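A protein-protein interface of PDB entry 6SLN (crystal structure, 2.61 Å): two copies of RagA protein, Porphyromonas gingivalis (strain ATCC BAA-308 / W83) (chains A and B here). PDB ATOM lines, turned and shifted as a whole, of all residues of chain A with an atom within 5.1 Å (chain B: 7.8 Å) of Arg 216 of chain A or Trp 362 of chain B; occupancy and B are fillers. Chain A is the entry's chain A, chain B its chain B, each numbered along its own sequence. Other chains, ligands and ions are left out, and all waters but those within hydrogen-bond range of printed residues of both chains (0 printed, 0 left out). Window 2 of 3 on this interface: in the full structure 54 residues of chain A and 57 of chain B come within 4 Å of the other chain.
O of Ile 359 of chain B lies within hydrogen-bond range of N of Gly 217 of chain A (3.0 Å).
The chain-end carboxylate (OXT) of Phe 997 of chain A lies within salt-bridge range of the guanidinium group (NH2) of Arg 216 of chain A. N of Ile 219 of chain A lies within hydrogen-bond range of O of Phe 997 of chain A (2.9 Å). The guanidinium group of Arg 358 of chain B is in hydrogen-bond range of the backbone carbonyl oxygen of Asn 360 of chain B (3.3 Å). The side-chain amide oxygen (OD1) of Asn 360 of chain B sits close to the backbone NH (N) of Trp 362 of chain B. The side-chain amide oxygen (OD1) of Asn 360 of chain B lies within hydrogen-bond range of the backbone NH (N) of Leu 363 of chain B (2.9 Å). The backbone NH of Thr 451 of chain B is in hydrogen-bond range of the backbone carbonyl oxygen of Trp 362 of chain B.
Among the printed residues, merely in contact across the chains: Arg 216 of chain A with Ile 359 of chain B, Arg 216 of chain A with Asn 360 of chain B, Arg 216 of chain A with Trp 362 of chain B, Ile 219 of chain A with Asn 360 of chain B, Ile 219 of chain A with Leu 363 of chain B, Val 948 of chain A with Trp 362 of chain B and Phe 997 of chain A with Asn 360 of chain B.
Arg 216 of chain A touches just these residues of chain B: Ile 359, Asn 360 and Trp 362. Of the printed residues of chain B, Val 948 of chain A touches Trp 362 (3.6 Å). Of the printed residues of chain A, Leu 363 of chain B touches Ile 219. Of the printed residues of chain B, Ile 219 of chain A touches Asn 360 and Leu 363. The nearest residue of chain B that does not touch Arg 216 of chain A is Glu 361 of chain B (5.4 Å). The nearest printed residue of chain A that does not touch Trp 362 of chain B is Asn 947 of chain A (4.1 Å).
Printed residues of chain A that touch a printed residue of chain B: Arg 216, Gly 217, Ile 219, Val 948 and Phe 997. Hydrophobic or aromatic side chains of chain A that line the printed part of chain B: Ile 219 and Val 948. Of the 17 printed residues of chain B, 4 touch a printed residue of chain A. Hydrophobic or aromatic side chains of chain B within 4 Å of the printed part of chain A: Ile 359, Trp 362 and Leu 363.
No position is printed for both chains.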
ATOM      1  N   SER A 214       4.387  -5.059 -29.939  1.00  0.00           N
ATOM      2  CA  SER A 214       3.794  -6.279 -29.381  1.00  0.00           C
ATOM      3  C   SER A 214       2.593  -6.022 -28.472  1.00  0.00           C
ATOM      4  O   SER A 214       2.702  -5.355 -27.433  1.00  0.00           O
ATOM      5  CB  SER A 214       4.828  -7.134 -28.641  1.00  0.00           C
ATOM      6  OG  SER A 214       5.799  -7.631 -29.551  1.00  0.00           O
ATOM      7  N   GLU A 215       1.439  -6.561 -28.898  1.00  0.00           N
ATOM      8  CA  GLU A 215       0.176  -6.714 -28.143  1.00  0.00           C
ATOM      9  C   GLU A 215      -0.281  -5.349 -27.638  1.00  0.00           C
ATOM     10  O   GLU A 215      -0.384  -4.408 -28.451  1.00  0.00           O
ATOM     11  CB  GLU A 215       0.356  -7.792 -27.075  1.00  0.00           C
ATOM     12  CG  GLU A 215       0.436  -9.222 -27.611  1.00  0.00           C
ATOM     13  CD  GLU A 215       1.866  -9.786 -27.611  1.00  0.00           C
ATOM     14  OE1 GLU A 215       2.048 -11.031 -27.519  1.00  0.00           O
ATOM     15  OE2 GLU A 215       2.814  -8.975 -27.718  1.00  0.00           O
ATOM     16  N   ARG A 216      -0.595  -5.184 -26.353  1.00  0.00           N
ATOM     17  CA  ARG A 216      -1.291  -3.998 -25.865  1.00  0.00           C
ATOM     18  C   ARG A 216      -0.461  -2.737 -26.079  1.00  0.00           C
ATOM     19  O   ARG A 216       0.738  -2.695 -25.772  1.00  0.00           O
ATOM     20  CB  ARG A 216      -1.628  -4.156 -24.379  1.00  0.00           C
ATOM     21  CG  ARG A 216      -2.724  -3.221 -23.880  1.00  0.00           C
ATOM     22  CD  ARG A 216      -2.829  -3.269 -22.367  1.00  0.00           C
ATOM     23  NE  ARG A 216      -3.814  -2.318 -21.855  1.00  0.00           N
ATOM     24  CZ  ARG A 216      -4.980  -2.660 -21.313  1.00  0.00           C
ATOM     25  NH1 ARG A 216      -5.329  -3.939 -21.194  1.00  0.00           N
ATOM     26  NH2 ARG A 216      -5.800  -1.712 -20.886  1.00  0.00           N
ATOM     27  N   GLY A 217      -1.111  -1.705 -26.606  1.00  0.00           N
ATOM     28  CA  GLY A 217      -0.509  -0.394 -26.711  1.00  0.00           C
ATOM     29  C   GLY A 217      -0.330   0.230 -25.338  1.00  0.00           C
ATOM     30  O   GLY A 217      -0.734  -0.311 -24.308  1.00  0.00           O
ATOM     31  N   ARG A 218       0.311   1.396 -25.326  1.00  0.00           N
ATOM     32  CA  ARG A 218       0.576   2.107 -24.083  1.00  0.00           C
ATOM     33  C   ARG A 218       0.093   3.543 -24.214  1.00  0.00           C
ATOM     34  O   ARG A 218       0.412   4.220 -25.197  1.00  0.00           O
ATOM     35  CB  ARG A 218       2.068   2.092 -23.710  1.00  0.00           C
ATOM     36  CG  ARG A 218       2.349   2.813 -22.392  1.00  0.00           C
ATOM     37  CD  ARG A 218       3.811   3.140 -22.189  1.00  0.00           C
ATOM     38  NE  ARG A 218       4.668   2.319 -23.030  1.00  0.00           N
ATOM     39  CZ  ARG A 218       5.992   2.391 -23.033  1.00  0.00           C
ATOM     40  NH1 ARG A 218       6.612   3.249 -22.230  1.00  0.00           N
ATOM     41  NH2 ARG A 218       6.695   1.605 -23.843  1.00  0.00           N
ATOM     42  N   ILE A 219      -0.678   4.001 -23.225  1.00  0.00           N
ATOM     43  CA  ILE A 219      -1.133   5.383 -23.139  1.00  0.00           C
ATOM     44  C   ILE A 219      -0.512   6.018 -21.905  1.00  0.00           C
ATOM     45  O   ILE A 219      -0.443   5.390 -20.841  1.00  0.00           O
ATOM     46  CB  ILE A 219      -2.668   5.475 -23.070  1.00  0.00           C
ATOM     47  CG1 ILE A 219      -3.300   4.597 -24.147  1.00  0.00           C
ATOM     48  CG2 ILE A 219      -3.107   6.924 -23.195  1.00  0.00           C
ATOM     49  CD1 ILE A 219      -4.734   4.227 -23.851  1.00  0.00           C
ATOM     50  N   ASN A 947      -8.609  -3.012 -14.428  1.00  0.00           N
ATOM     51  CA  ASN A 947      -7.969  -3.304 -15.702  1.00  0.00           C
ATOM     52  C   ASN A 947      -7.818  -2.104 -16.623  1.00  0.00           C
ATOM     53  O   ASN A 947      -7.275  -2.269 -17.718  1.00  0.00           O
ATOM     54  CB  ASN A 947      -8.741  -4.416 -16.424  1.00  0.00           C
ATOM     55  CG  ASN A 947      -7.985  -4.960 -17.605  1.00  0.00           C
ATOM     56  OD1 ASN A 947      -6.755  -4.975 -17.610  1.00  0.00           O
ATOM     57  ND2 ASN A 947      -8.711  -5.387 -18.628  1.00  0.00           N
ATOM     58  N   VAL A 948      -8.267  -0.912 -16.242  1.00  0.00           N
ATOM     59  CA  VAL A 948      -8.011   0.256 -17.081  1.00  0.00           C
ATOM     60  C   VAL A 948      -6.602   0.766 -16.797  1.00  0.00           C
ATOM     61  O   VAL A 948      -5.691   0.573 -17.610  1.00  0.00           O
ATOM     62  CB  VAL A 948      -9.064   1.364 -16.874  1.00  0.00           C
ATOM     63  CG1 VAL A 948      -8.640   2.642 -17.574  1.00  0.00           C
ATOM     64  CG2 VAL A 948     -10.415   0.917 -17.400  1.00  0.00           C
ATOM     65  N   PHE A 997      -1.823   3.758 -18.719  1.00  0.00           N
ATOM     66  CA  PHE A 997      -2.684   2.610 -18.966  1.00  0.00           C
ATOM     67  C   PHE A 997      -2.617   2.127 -20.404  1.00  0.00           C
ATOM     68  O   PHE A 997      -1.628   2.359 -21.093  1.00  0.00           O
ATOM     69  CB  PHE A 997      -4.127   2.923 -18.578  1.00  0.00           C
ATOM     70  CG  PHE A 997      -4.579   4.296 -18.944  1.00  0.00           C
ATOM     71  CD1 PHE A 997      -4.721   4.650 -20.265  1.00  0.00           C
ATOM     72  CD2 PHE A 997      -4.908   5.219 -17.960  1.00  0.00           C
ATOM     73  CE1 PHE A 997      -5.160   5.905 -20.609  1.00  0.00           C
ATOM     74  CE2 PHE A 997      -5.345   6.478 -18.289  1.00  0.00           C
ATOM     75  CZ  PHE A 997      -5.472   6.828 -19.619  1.00  0.00           C
ATOM     76  OXT PHE A 997      -3.535   1.471 -20.892  1.00  0.00           O
ATOM     77  N   GLN B 323      -2.642  -6.424 -37.062  1.00  0.00           N
ATOM     78  CA  GLN B 323      -3.037  -6.631 -35.673  1.00  0.00           C
ATOM     79  C   GLN B 323      -3.518  -5.318 -35.043  1.00  0.00           C
ATOM     80  O   GLN B 323      -2.837  -4.686 -34.236  1.00  0.00           O
ATOM     81  CB  GLN B 323      -1.847  -7.226 -34.923  1.00  0.00           C
ATOM     82  CG  GLN B 323      -2.007  -7.456 -33.425  1.00  0.00           C
ATOM     83  CD  GLN B 323      -1.291  -8.704 -32.931  1.00  0.00           C
ATOM     84  OE1 GLN B 323      -1.876  -9.545 -32.252  1.00  0.00           O
ATOM     85  NE2 GLN B 323      -0.016  -8.825 -33.274  1.00  0.00           N
ATOM     86  N   ARG B 358      -6.208  -0.236 -32.681  1.00  0.00           N
ATOM     87  CA  ARG B 358      -6.912  -0.731 -31.503  1.00  0.00           C
ATOM     88  C   ARG B 358      -5.889  -0.830 -30.388  1.00  0.00           C
ATOM     89  O   ARG B 358      -5.152  -1.811 -30.293  1.00  0.00           O
ATOM     90  CB  ARG B 358      -7.560  -2.083 -31.767  1.00  0.00           C
ATOM     91  CG  ARG B 358      -8.534  -2.507 -30.680  1.00  0.00           C
ATOM     92  CD  ARG B 358      -9.949  -2.052 -31.033  1.00  0.00           C
ATOM     93  NE  ARG B 358     -10.780  -1.770 -29.865  1.00  0.00           N
ATOM     94  CZ  ARG B 358     -11.940  -1.116 -29.915  1.00  0.00           C
ATOM     95  NH1 ARG B 358     -12.407  -0.671 -31.077  1.00  0.00           N
ATOM     96  NH2 ARG B 358     -12.634  -0.909 -28.803  1.00  0.00           N
ATOM     97  N   ILE B 359      -5.837   0.188 -29.532  1.00  0.00           N
ATOM     98  CA  ILE B 359      -4.772   0.210 -28.541  1.00  0.00           C
ATOM     99  C   ILE B 359      -5.042  -0.776 -27.409  1.00  0.00           C
ATOM    100  O   ILE B 359      -4.094  -1.317 -26.823  1.00  0.00           O
ATOM    101  CB  ILE B 359      -4.553   1.641 -28.028  1.00  0.00           C
ATOM    102  CG1 ILE B 359      -4.122   2.522 -29.197  1.00  0.00           C
ATOM    103  CG2 ILE B 359      -3.495   1.654 -26.948  1.00  0.00           C
ATOM    104  CD1 ILE B 359      -3.293   3.698 -28.793  1.00  0.00           C
ATOM    105  N   ASN B 360      -6.307  -1.049 -27.100  1.00  0.00           N
ATOM    106  CA  ASN B 360      -6.655  -2.086 -26.129  1.00  0.00           C
ATOM    107  C   ASN B 360      -8.132  -2.428 -26.292  1.00  0.00           C
ATOM    108  O   ASN B 360      -8.786  -2.019 -27.259  1.00  0.00           O
ATOM    109  CB  ASN B 360      -6.330  -1.656 -24.696  1.00  0.00           C
ATOM    110  CG  ASN B 360      -6.864  -0.275 -24.369  1.00  0.00           C
ATOM    111  OD1 ASN B 360      -8.041   0.012 -24.589  1.00  0.00           O
ATOM    112  ND2 ASN B 360      -5.996   0.594 -23.854  1.00  0.00           N
ATOM    113  N   GLU B 361      -8.655  -3.170 -25.316  1.00  0.00           N
ATOM    114  CA  GLU B 361     -10.002  -3.720 -25.409  1.00  0.00           C
ATOM    115  C   GLU B 361     -11.038  -2.624 -25.597  1.00  0.00           C
ATOM    116  O   GLU B 361     -12.034  -2.813 -26.302  1.00  0.00           O
ATOM    117  CB  GLU B 361     -10.306  -4.552 -24.155  1.00  0.00           C
ATOM    118  CG  GLU B 361     -11.624  -5.324 -24.239  1.00  0.00           C
ATOM    119  CD  GLU B 361     -12.143  -5.817 -22.888  1.00  0.00           C
ATOM    120  OE1 GLU B 361     -11.525  -6.749 -22.342  1.00  0.00           O
ATOM    121  OE2 GLU B 361     -13.163  -5.295 -22.379  1.00  0.00           O
ATOM    122  N   TRP B 362     -10.813  -1.466 -24.985  1.00  0.00           N
ATOM    123  CA  TRP B 362     -11.817  -0.416 -24.974  1.00  0.00           C
ATOM    124  C   TRP B 362     -11.489   0.778 -25.864  1.00  0.00           C
ATOM    125  O   TRP B 362     -12.398   1.558 -26.175  1.00  0.00           O
ATOM    126  CB  TRP B 362     -12.053   0.076 -23.532  1.00  0.00           C
ATOM    127  CG  TRP B 362     -11.124   1.174 -23.091  1.00  0.00           C
ATOM    128  CD1 TRP B 362     -11.211   2.517 -23.391  1.00  0.00           C
ATOM    129  CD2 TRP B 362      -9.969   1.028 -22.269  1.00  0.00           C
ATOM    130  NE1 TRP B 362     -10.173   3.203 -22.810  1.00  0.00           N
ATOM    131  CE2 TRP B 362      -9.395   2.314 -22.116  1.00  0.00           C
ATOM    132  CE3 TRP B 362      -9.360  -0.063 -21.652  1.00  0.00           C
ATOM    133  CZ2 TRP B 362      -8.246   2.532 -21.370  1.00  0.00           C
ATOM    134  CZ3 TRP B 362      -8.221   0.154 -20.907  1.00  0.00           C
ATOM    135  CH2 TRP B 362      -7.670   1.441 -20.774  1.00  0.00           C
ATOM    136  N   LEU B 363     -10.234   0.950 -26.289  1.00  0.00           N
ATOM    137  CA  LEU B 363      -9.821   2.176 -26.973  1.00  0.00           C
ATOM    138  C   LEU B 363      -9.282   1.895 -28.372  1.00  0.00           C
ATOM    139  O   LEU B 363      -8.311   1.146 -28.535  1.00  0.00           O
ATOM    140  CB  LEU B 363      -8.766   2.940 -26.173  1.00  0.00           C
ATOM    141  CG  LEU B 363      -8.403   4.254 -26.866  1.00  0.00           C
ATOM    142  CD1 LEU B 363      -9.603   5.192 -26.878  1.00  0.00           C
ATOM    143  CD2 LEU B 363      -7.219   4.920 -26.214  1.00  0.00           C
ATOM    144  N   LYS B 364      -9.893   2.536 -29.368  1.00  0.00           N
ATOM    145  CA  LYS B 364      -9.335   2.674 -30.707  1.00  0.00           C
ATOM    146  C   LYS B 364      -9.118   4.158 -30.975  1.00  0.00           C
ATOM    147  O   LYS B 364      -9.986   4.979 -30.670  1.00  0.00           O
ATOM    148  CB  LYS B 364     -10.264   2.053 -31.765  1.00  0.00           C
ATOM    149  CG  LYS B 364      -9.866   2.348 -33.214  1.00  0.00           C
ATOM    150  CD  LYS B 364     -10.754   1.606 -34.232  1.00  0.00           C
ATOM    151  CE  LYS B 364     -10.686   2.287 -35.612  1.00  0.00           C
ATOM    152  NZ  LYS B 364     -11.334   1.512 -36.716  1.00  0.00           N
ATOM    153  N   VAL B 365      -7.955   4.506 -31.514  1.00  0.00           N
ATOM    154  CA  VAL B 365      -7.624   5.887 -31.841  1.00  0.00           C
ATOM    155  C   VAL B 365      -7.193   5.932 -33.298  1.00  0.00           C
ATOM    156  O   VAL B 365      -6.957   4.903 -33.932  1.00  0.00           O
ATOM    157  CB  VAL B 365      -6.515   6.463 -30.942  1.00  0.00           C
ATOM    158  CG1 VAL B 365      -6.909   6.354 -29.473  1.00  0.00           C
ATOM    159  CG2 VAL B 365      -5.178   5.758 -31.222  1.00  0.00           C
ATOM    160  N   ALA B 448     -10.737   9.539 -30.801  1.00  0.00           N
ATOM    161  CA  ALA B 448     -10.700   8.452 -29.844  1.00  0.00           C
ATOM    162  C   ALA B 448     -12.042   7.749 -29.907  1.00  0.00           C
ATOM    163  O   ALA B 448     -13.083   8.404 -30.012  1.00  0.00           O
ATOM    164  CB  ALA B 448     -10.421   8.965 -28.431  1.00  0.00           C
ATOM    165  N   GLN B 449     -12.021   6.419 -29.880  1.00  0.00           N
ATOM    166  CA  GLN B 449     -13.245   5.621 -29.887  1.00  0.00           C
ATOM    167  C   GLN B 449     -13.233   4.713 -28.660  1.00  0.00           C
ATOM    168  O   GLN B 449     -12.528   3.698 -28.627  1.00  0.00           O
ATOM    169  CB  GLN B 449     -13.380   4.824 -31.180  1.00  0.00           C
ATOM    170  CG  GLN B 449     -14.820   4.703 -31.654  1.00  0.00           C
ATOM    171  CD  GLN B 449     -14.995   3.612 -32.682  1.00  0.00           C
ATOM    172  OE1 GLN B 449     -14.735   2.440 -32.398  1.00  0.00           O
ATOM    173  NE2 GLN B 449     -15.430   3.986 -33.889  1.00  0.00           N
ATOM    174  N   ILE B 450     -14.033   5.075 -27.658  1.00  0.00           N
ATOM    175  CA  ILE B 450     -14.097   4.362 -26.386  1.00  0.00           C
ATOM    176  C   ILE B 450     -15.387   3.562 -26.333  1.00  0.00           C
ATOM    177  O   ILE B 450     -16.485   4.129 -26.423  1.00  0.00           O
ATOM    178  CB  ILE B 450     -14.024   5.323 -25.195  1.00  0.00           C
ATOM    179  CG1 ILE B 450     -12.755   6.169 -25.259  1.00  0.00           C
ATOM    180  CG2 ILE B 450     -14.052   4.537 -23.940  1.00  0.00           C
ATOM    181  CD1 ILE B 450     -12.957   7.578 -24.739  1.00  0.00           C
ATOM    182  N   THR B 451     -15.258   2.248 -26.150  1.00  0.00           N
ATOM    183  CA  THR B 451     -16.396   1.338 -26.026  1.00  0.00           C
ATOM    184  C   THR B 451     -16.375   0.744 -24.620  1.00  0.00           C
ATOM    185  O   THR B 451     -15.765  -0.312 -24.404  1.00  0.00           O
ATOM    186  CB  THR B 451     -16.336   0.245 -27.097  1.00  0.00           C
ATOM    187  OG1 THR B 451     -15.334  -0.715 -26.746  1.00  0.00           O
ATOM    188  CG2 THR B 451     -15.977   0.835 -28.457  1.00  0.00           C
ATOM    189  N   PRO B 452     -17.007   1.395 -23.630  1.00  0.00           N
ATOM    190  CA  PRO B 452     -16.866   0.943 -22.230  1.00  0.00           C
ATOM    191  C   PRO B 452     -17.736  -0.246 -21.843  1.00  0.00           C
ATOM    192  O   PRO B 452     -17.340  -1.003 -20.944  1.00  0.00           O
ATOM    193  CB  PRO B 452     -17.264   2.186 -21.419  1.00  0.00           C
ATOM    194  CG  PRO B 452     -18.142   2.964 -22.325  1.00  0.00           C
ATOM    195  CD  PRO B 452     -17.636   2.720 -23.722  1.00  0.00           C
ATOM    196  N   ILE B 453     -18.906  -0.419 -22.471  1.00  0.00           N
ATOM    197  CA  ILE B 453     -19.775  -1.577 -22.295  1.00  0.00           C
ATOM    198  C   ILE B 453     -20.376  -1.945 -23.643  1.00  0.00           C
ATOM    199  O   ILE B 453     -20.171  -1.257 -24.643  1.00  0.00           O
ATOM    200  CB  ILE B 453     -20.890  -1.322 -21.268  1.00  0.00           C
ATOM    201  CG1 ILE B 453     -21.703  -0.094 -21.676  1.00  0.00           C
ATOM    202  CG2 ILE B 453     -20.324  -1.188 -19.873  1.00  0.00           C
ATOM    203  CD1 ILE B 453     -22.641   0.441 -20.560  1.00  0.00           C
ATOM    204  N   LEU B 456     -22.197   0.536 -26.298  1.00  0.00           N
ATOM    205  CA  LEU B 456     -21.874   1.932 -26.018  1.00  0.00           C
ATOM    206  C   LEU B 456     -20.586   2.319 -26.741  1.00  0.00           C
ATOM    207  O   LEU B 456     -19.494   1.922 -26.322  1.00  0.00           O
ATOM    208  CB  LEU B 456     -21.727   2.157 -24.516  1.00  0.00           C
ATOM    209  CG  LEU B 456     -21.801   3.644 -24.178  1.00  0.00           C
ATOM    210  CD1 LEU B 456     -23.141   4.229 -24.608  1.00  0.00           C
ATOM    211  CD2 LEU B 456     -21.541   3.887 -22.713  1.00  0.00           C
ATOM    212  N   LEU B 458     -18.565   5.639 -27.587  1.00  0.00           N
ATOM    213  CA  LEU B 458     -18.310   7.064 -27.409  1.00  0.00           C
ATOM    214  C   LEU B 458     -17.158   7.476 -28.323  1.00  0.00           C
ATOM    215  O   LEU B 458     -16.048   6.943 -28.198  1.00  0.00           O
ATOM    216  CB  LEU B 458     -17.978   7.378 -25.949  1.00  0.00           C
ATOM    217  CG  LEU B 458     -19.072   7.153 -24.894  1.00  0.00           C
ATOM    218  CD1 LEU B 458     -19.038   5.743 -24.436  1.00  0.00           C
ATOM    219  CD2 LEU B 458     -18.894   8.056 -23.702  1.00  0.00           C
